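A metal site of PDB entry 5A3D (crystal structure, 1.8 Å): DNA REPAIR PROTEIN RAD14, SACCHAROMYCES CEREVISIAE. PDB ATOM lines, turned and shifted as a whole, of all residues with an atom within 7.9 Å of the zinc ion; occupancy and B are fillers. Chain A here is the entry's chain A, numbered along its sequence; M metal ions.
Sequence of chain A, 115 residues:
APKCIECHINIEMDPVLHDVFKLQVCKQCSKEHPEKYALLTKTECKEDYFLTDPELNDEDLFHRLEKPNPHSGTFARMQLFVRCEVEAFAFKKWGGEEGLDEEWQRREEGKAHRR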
ATOM      1  N   LYS A   3     -27.419  30.468 -15.389  1.00  0.00           N
ATOM      2  CA  LYS A   3     -26.330  30.138 -14.471  1.00  0.00           C
ATOM      3  C   LYS A   3     -26.702  29.049 -13.511  1.00  0.00           C
ATOM      4  O   LYS A   3     -27.893  28.842 -13.197  1.00  0.00           O
ATOM      5  CB  LYS A   3     -25.885  31.333 -13.640  1.00  0.00           C
ATOM      6  CG  LYS A   3     -25.635  32.635 -14.449  1.00  0.00           C
ATOM      7  CD  LYS A   3     -24.380  32.638 -15.312  1.00  0.00           C
ATOM      8  CE  LYS A   3     -24.262  33.917 -16.197  1.00  0.00           C
ATOM      9  NZ  LYS A   3     -23.346  35.004 -15.740  1.00  0.00           N
ATOM     10  N   CYS A   4     -25.690  28.303 -13.079  1.00  0.00           N
ATOM     11  CA  CYS A   4     -25.869  27.325 -12.019  1.00  0.00           C
ATOM     12  C   CYS A   4     -26.518  27.909 -10.747  1.00  0.00           C
ATOM     13  O   CYS A   4     -26.154  28.963 -10.262  1.00  0.00           O
ATOM     14  CB  CYS A   4     -24.526  26.685 -11.670  1.00  0.00           C
ATOM     15  SG  CYS A   4     -24.521  25.717 -10.164  1.00  0.00           S
ATOM     16  N   ILE A   5     -27.556  27.225 -10.240  1.00  0.00           N
ATOM     17  CA  ILE A   5     -28.301  27.724  -9.083  1.00  0.00           C
ATOM     18  C   ILE A   5     -27.493  27.645  -7.756  1.00  0.00           C
ATOM     19  O   ILE A   5     -27.836  28.271  -6.765  1.00  0.00           O
ATOM     20  CB  ILE A   5     -29.645  26.965  -8.939  1.00  0.00           C
ATOM     21  CG1 ILE A   5     -29.412  25.530  -8.496  1.00  0.00           C
ATOM     22  CG2 ILE A   5     -30.382  26.921 -10.292  1.00  0.00           C
ATOM     23  CD1 ILE A   5     -30.687  24.684  -8.276  1.00  0.00           C
ATOM     24  N   GLU A   6     -26.390  26.889  -7.721  1.00  0.00           N
ATOM     25  CA  GLU A   6     -25.515  26.986  -6.526  1.00  0.00           C
ATOM     26  C   GLU A   6     -24.466  28.091  -6.611  1.00  0.00           C
ATOM     27  O   GLU A   6     -24.402  28.961  -5.692  1.00  0.00           O
ATOM     28  CB  GLU A   6     -24.837  25.656  -6.229  1.00  0.00           C
ATOM     29  CG  GLU A   6     -25.820  24.588  -5.891  1.00  0.00           C
ATOM     30  CD  GLU A   6     -26.448  24.755  -4.502  1.00  0.00           C
ATOM     31  OE1 GLU A   6     -25.889  25.495  -3.622  1.00  0.00           O
ATOM     32  OE2 GLU A   6     -27.503  24.172  -4.321  1.00  0.00           O
ATOM     33  N   CYS A   7     -23.639  28.085  -7.665  1.00  0.00           N
ATOM     34  CA  CYS A   7     -22.563  29.024  -7.720  1.00  0.00           C
ATOM     35  C   CYS A   7     -22.942  30.411  -8.316  1.00  0.00           C
ATOM     36  O   CYS A   7     -22.273  31.446  -8.001  1.00  0.00           O
ATOM     37  CB  CYS A   7     -21.298  28.391  -8.391  1.00  0.00           C
ATOM     38  SG  CYS A   7     -21.429  28.033 -10.093  1.00  0.00           S
ATOM     39  N   HIS A   8     -23.910  30.416  -9.226  1.00  0.00           N
ATOM     40  CA  HIS A   8     -24.319  31.628  -9.976  1.00  0.00           C
ATOM     41  C   HIS A   8     -23.261  32.124 -11.017  1.00  0.00           C
ATOM     42  O   HIS A   8     -23.314  33.231 -11.495  1.00  0.00           O
ATOM     43  CB  HIS A   8     -24.705  32.752  -9.006  1.00  0.00           C
ATOM     44  CG  HIS A   8     -25.698  32.321  -7.990  1.00  0.00           C
ATOM     45  ND1 HIS A   8     -26.973  31.882  -8.328  1.00  0.00           N
ATOM     46  CD2 HIS A   8     -25.599  32.190  -6.642  1.00  0.00           C
ATOM     47  CE1 HIS A   8     -27.602  31.509  -7.219  1.00  0.00           C
ATOM     48  NE2 HIS A   8     -26.798  31.721  -6.189  1.00  0.00           N
ATOM     49  N   ILE A   9     -22.380  31.210 -11.372  1.00  0.00           N
ATOM     50  CA  ILE A   9     -21.199  31.443 -12.174  1.00  0.00           C
ATOM     51  C   ILE A   9     -21.130  30.612 -13.405  1.00  0.00           C
ATOM     52  O   ILE A   9     -21.108  31.176 -14.522  1.00  0.00           O
ATOM     53  CB  ILE A   9     -19.962  31.230 -11.314  1.00  0.00           C
ATOM     54  CG1 ILE A   9     -20.095  32.232 -10.165  1.00  0.00           C
ATOM     55  CG2 ILE A   9     -18.689  31.427 -12.134  1.00  0.00           C
ATOM     56  CD1 ILE A   9     -18.848  32.704  -9.571  1.00  0.00           C
ATOM     57  N   ASN A  10     -21.016  29.296 -13.214  1.00  0.00           N
ATOM     58  CA  ASN A  10     -20.915  28.363 -14.310  1.00  0.00           C
ATOM     59  C   ASN A  10     -22.223  28.322 -15.116  1.00  0.00           C
ATOM     60  O   ASN A  10     -23.350  28.480 -14.541  1.00  0.00           O
ATOM     61  CB  ASN A  10     -20.575  26.987 -13.794  1.00  0.00           C
ATOM     62  CG  ASN A  10     -19.082  26.751 -13.673  1.00  0.00           C
ATOM     63  OD1 ASN A  10     -18.257  27.319 -14.461  1.00  0.00           O
ATOM     64  ND2 ASN A  10     -18.729  25.897 -12.729  1.00  0.00           N
ATOM     65  N   ILE A  11     -22.056  28.190 -16.431  1.00  0.00           N
ATOM     66  CA  ILE A  11     -23.141  28.009 -17.386  1.00  0.00           C
ATOM     67  C   ILE A  11     -23.138  26.589 -18.015  1.00  0.00           C
ATOM     68  O   ILE A  11     -24.002  26.266 -18.879  1.00  0.00           O
ATOM     69  CB  ILE A  11     -23.086  29.056 -18.528  1.00  0.00           C
ATOM     70  CG1 ILE A  11     -21.816  28.920 -19.384  1.00  0.00           C
ATOM     71  CG2 ILE A  11     -23.270  30.477 -18.001  1.00  0.00           C
ATOM     72  CD1 ILE A  11     -21.745  29.908 -20.502  1.00  0.00           C
ATOM     73  N   GLU A  12     -22.149  25.750 -17.679  1.00  0.00           N
ATOM     74  CA  GLU A  12     -22.100  24.387 -18.208  1.00  0.00           C
ATOM     75  C   GLU A  12     -22.629  23.505 -17.074  1.00  0.00           C
ATOM     76  O   GLU A  12     -21.964  23.362 -16.047  1.00  0.00           O
ATOM     77  CB  GLU A  12     -20.706  23.956 -18.636  1.00  0.00           C
ATOM     78  CG  GLU A  12     -20.097  24.849 -19.684  1.00  0.00           C
ATOM     79  CD  GLU A  12     -20.058  24.291 -21.082  1.00  0.00           C
ATOM     80  OE1 GLU A  12     -20.069  23.005 -21.226  1.00  0.00           O
ATOM     81  OE2 GLU A  12     -19.961  25.123 -22.046  1.00  0.00           O
ATOM     82  N   MET A  13     -23.831  22.932 -17.258  1.00  0.00           N
ATOM     83  CA  MET A  13     -24.425  22.159 -16.145  1.00  0.00           C
ATOM     84  C   MET A  13     -23.932  20.729 -16.195  1.00  0.00           C
ATOM     85  O   MET A  13     -23.564  20.223 -17.251  1.00  0.00           O
ATOM     86  CB  MET A  13     -25.955  22.232 -16.236  1.00  0.00           C
ATOM     87  CG  MET A  13     -26.519  23.628 -16.330  1.00  0.00           C
ATOM     88  SD  MET A  13     -25.965  24.598 -14.868  1.00  0.00           S
ATOM     89  CE  MET A  13     -26.024  26.229 -15.678  1.00  0.00           C
ATOM     90  N   GLN A  24     -30.464  22.653 -12.678  1.00  0.00           N
ATOM     91  CA  GLN A  24     -29.439  23.524 -13.292  1.00  0.00           C
ATOM     92  C   GLN A  24     -28.253  23.734 -12.373  1.00  0.00           C
ATOM     93  O   GLN A  24     -28.194  24.823 -11.693  1.00  0.00           O
ATOM     94  CB  GLN A  24     -30.023  24.926 -13.630  1.00  0.00           C
ATOM     95  CG  GLN A  24     -31.184  24.851 -14.576  1.00  0.00           C
ATOM     96  CD  GLN A  24     -30.787  24.521 -16.022  1.00  0.00           C
ATOM     97  OE1 GLN A  24     -29.628  24.737 -16.462  1.00  0.00           O
ATOM     98  NE2 GLN A  24     -31.780  24.072 -16.787  1.00  0.00           N
ATOM     99  N   VAL A  25     -27.454  22.680 -12.253  1.00  0.00           N
ATOM    100  CA  VAL A  25     -26.329  22.589 -11.262  1.00  0.00           C
ATOM    101  C   VAL A  25     -25.092  22.096 -11.989  1.00  0.00           C
ATOM    102  O   VAL A  25     -25.189  21.180 -12.732  1.00  0.00           O
ATOM    103  CB  VAL A  25     -26.690  21.637 -10.088  1.00  0.00           C
ATOM    104  CG1 VAL A  25     -25.655  21.689  -8.986  1.00  0.00           C
ATOM    105  CG2 VAL A  25     -28.003  22.123  -9.470  1.00  0.00           C
ATOM    106  N   CYS A  26     -23.934  22.788 -11.848  1.00  0.00           N
ATOM    107  CA  CYS A  26     -22.691  22.397 -12.454  1.00  0.00           C
ATOM    108  C   CYS A  26     -22.091  21.255 -11.668  1.00  0.00           C
ATOM    109  O   CYS A  26     -22.395  21.010 -10.470  1.00  0.00           O
ATOM    110  CB  CYS A  26     -21.705  23.616 -12.596  1.00  0.00           C
ATOM    111  SG  CYS A  26     -21.017  24.157 -11.016  1.00  0.00           S
ATOM    112  N   LYS A  27     -21.152  20.626 -12.300  1.00  0.00           N
ATOM    113  CA  LYS A  27     -20.643  19.450 -11.750  1.00  0.00           C
ATOM    114  C   LYS A  27     -19.827  19.783 -10.480  1.00  0.00           C
ATOM    115  O   LYS A  27     -19.821  19.029  -9.549  1.00  0.00           O
ATOM    116  CB  LYS A  27     -19.806  18.851 -12.851  1.00  0.00           C
ATOM    117  CG  LYS A  27     -18.775  17.933 -12.346  1.00  0.00           C
ATOM    118  CD  LYS A  27     -19.299  16.611 -12.242  1.00  0.00           C
ATOM    119  CE  LYS A  27     -19.104  15.875 -13.564  1.00  0.00           C
ATOM    120  NZ  LYS A  27     -19.992  14.667 -13.359  1.00  0.00           N
ATOM    121  N   GLN A  28     -19.132  20.869 -10.484  1.00  0.00           N
ATOM    122  CA  GLN A  28     -18.256  21.247  -9.357  1.00  0.00           C
ATOM    123  C   GLN A  28     -19.114  21.461  -8.106  1.00  0.00           C
ATOM    124  O   GLN A  28     -18.805  20.937  -7.048  1.00  0.00           O
ATOM    125  CB  GLN A  28     -17.390  22.453  -9.705  1.00  0.00           C
ATOM    126  CG  GLN A  28     -16.604  23.039  -8.491  1.00  0.00           C
ATOM    127  CD  GLN A  28     -15.567  24.060  -8.852  1.00  0.00           C
ATOM    128  OE1 GLN A  28     -15.387  24.409  -9.979  1.00  0.00           O
ATOM    129  NE2 GLN A  28     -14.867  24.589  -7.805  1.00  0.00           N
ATOM    130  N   CYS A  29     -20.229  22.169  -8.265  1.00  0.00           N
ATOM    131  CA  CYS A  29     -21.160  22.405  -7.233  1.00  0.00           C
ATOM    132  C   CYS A  29     -21.846  21.136  -6.722  1.00  0.00           C
ATOM    133  O   CYS A  29     -22.093  20.988  -5.489  1.00  0.00           O
ATOM    134  CB  CYS A  29     -22.190  23.462  -7.644  1.00  0.00           C
ATOM    135  SG  CYS A  29     -21.521  25.143  -7.716  1.00  0.00           S
ATOM    136  N   SER A  30     -22.167  20.242  -7.638  1.00  0.00           N
ATOM    137  CA  SER A  30     -22.689  18.955  -7.266  1.00  0.00           C
ATOM    138  C   SER A  30     -21.670  18.165  -6.300  1.00  0.00           C
ATOM    139  O   SER A  30     -22.113  17.650  -5.291  1.00  0.00           O
ATOM    140  CB  SER A  30     -23.060  18.140  -8.458  1.00  0.00           C
ATOM    141  OG  SER A  30     -21.990  17.451  -9.066  1.00  0.00           O
ATOM    142  N   GLU A  32     -19.427  19.608  -4.381  1.00  0.00           N
ATOM    143  CA  GLU A  32     -19.324  20.465  -3.193  1.00  0.00           C
ATOM    144  C   GLU A  32     -20.570  20.417  -2.260  1.00  0.00           C
ATOM    145  O   GLU A  32     -20.521  20.764  -1.051  1.00  0.00           O
ATOM    146  CB  GLU A  32     -19.034  21.929  -3.612  1.00  0.00           C
ATOM    147  CG  GLU A  32     -17.652  22.093  -4.298  1.00  0.00           C
ATOM    148  CD  GLU A  32     -17.334  23.475  -4.925  1.00  0.00           C
ATOM    149  OE1 GLU A  32     -18.305  24.189  -5.339  1.00  0.00           O
ATOM    150  OE2 GLU A  32     -16.077  23.792  -5.110  1.00  0.00           O
ATOM    151  N   HIS A  33     -21.644  19.855  -2.762  1.00  0.00           N
ATOM    152  CA  HIS A  33     -22.885  19.787  -2.015  1.00  0.00           C
ATOM    153  C   HIS A  33     -23.555  18.440  -2.139  1.00  0.00           C
ATOM    154  O   HIS A  33     -24.659  18.330  -2.714  1.00  0.00           O
ATOM    155  CB  HIS A  33     -23.775  20.883  -2.508  1.00  0.00           C
ATOM    156  CG  HIS A  33     -23.226  22.234  -2.276  1.00  0.00           C
ATOM    157  ND1 HIS A  33     -23.148  22.781  -1.001  1.00  0.00           N
ATOM    158  CD2 HIS A  33     -22.658  23.130  -3.115  1.00  0.00           C
ATOM    159  CE1 HIS A  33     -22.606  23.985  -1.095  1.00  0.00           C
ATOM    160  NE2 HIS A  33     -22.335  24.228  -2.369  1.00  0.00           N
ATOM    161  N   TYR A  37     -26.920  16.653  -3.807  1.00  0.00           N
ATOM    162  CA  TYR A  37     -26.761  16.167  -5.162  1.00  0.00           C
ATOM    163  C   TYR A  37     -26.132  14.810  -5.358  1.00  0.00           C
ATOM    164  O   TYR A  37     -26.001  14.369  -6.468  1.00  0.00           O
ATOM    165  CB  TYR A  37     -25.993  17.181  -6.008  1.00  0.00           C
ATOM    166  CG  TYR A  37     -26.617  18.547  -5.985  1.00  0.00           C
ATOM    167  CD1 TYR A  37     -27.907  18.758  -6.418  1.00  0.00           C
ATOM    168  CD2 TYR A  37     -25.942  19.636  -5.449  1.00  0.00           C
ATOM    169  CE1 TYR A  37     -28.486  20.016  -6.414  1.00  0.00           C
ATOM    170  CE2 TYR A  37     -26.540  20.893  -5.421  1.00  0.00           C
ATOM    171  CZ  TYR A  37     -27.792  21.102  -5.888  1.00  0.00           C
ATOM    172  OH  TYR A  37     -28.336  22.382  -5.869  1.00  0.00           O
HETATM  173 ZN    ZN M   1     -22.135  25.724  -9.764  1.00  0.00          ZN
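Within 4 Å of the zinc ion: Cys 4, Cys 7, Cys 26 and Cys 29.
The nearest printed residue that does not touch the zinc ion is Glu 6 (4.4 Å).
The side-chain sulfur (SG) of Cys 26 lies close to the side-chain amide nitrogen (ND2) of Asn 10 (3.3 Å).
The side-chain sulfur of Cys 4 lies close to the backbone NH of Glu 6 (3.3 Å).
The backbone NH (N) of Cys 4 sits at hydrogen-bond distance from the backbone carbonyl oxygen (O) of Asn 10, at 2.8 Å.
SG of Cys 7 lies close to N of Asn 10 (3.4 Å).
SG of Cys 7 sits close to N of Ile 9.
The zinc ion is bound by the side-chain sulfur (SG) of Cys 29, at 2.2 Å.
The zinc ion is bound by SG of Cys 26, 2.3 Å away.
SG of Cys 4 binds the zinc ion.
The zinc ion is bound by the side-chain sulfur (SG) of Cys 7, at 2.4 Å.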
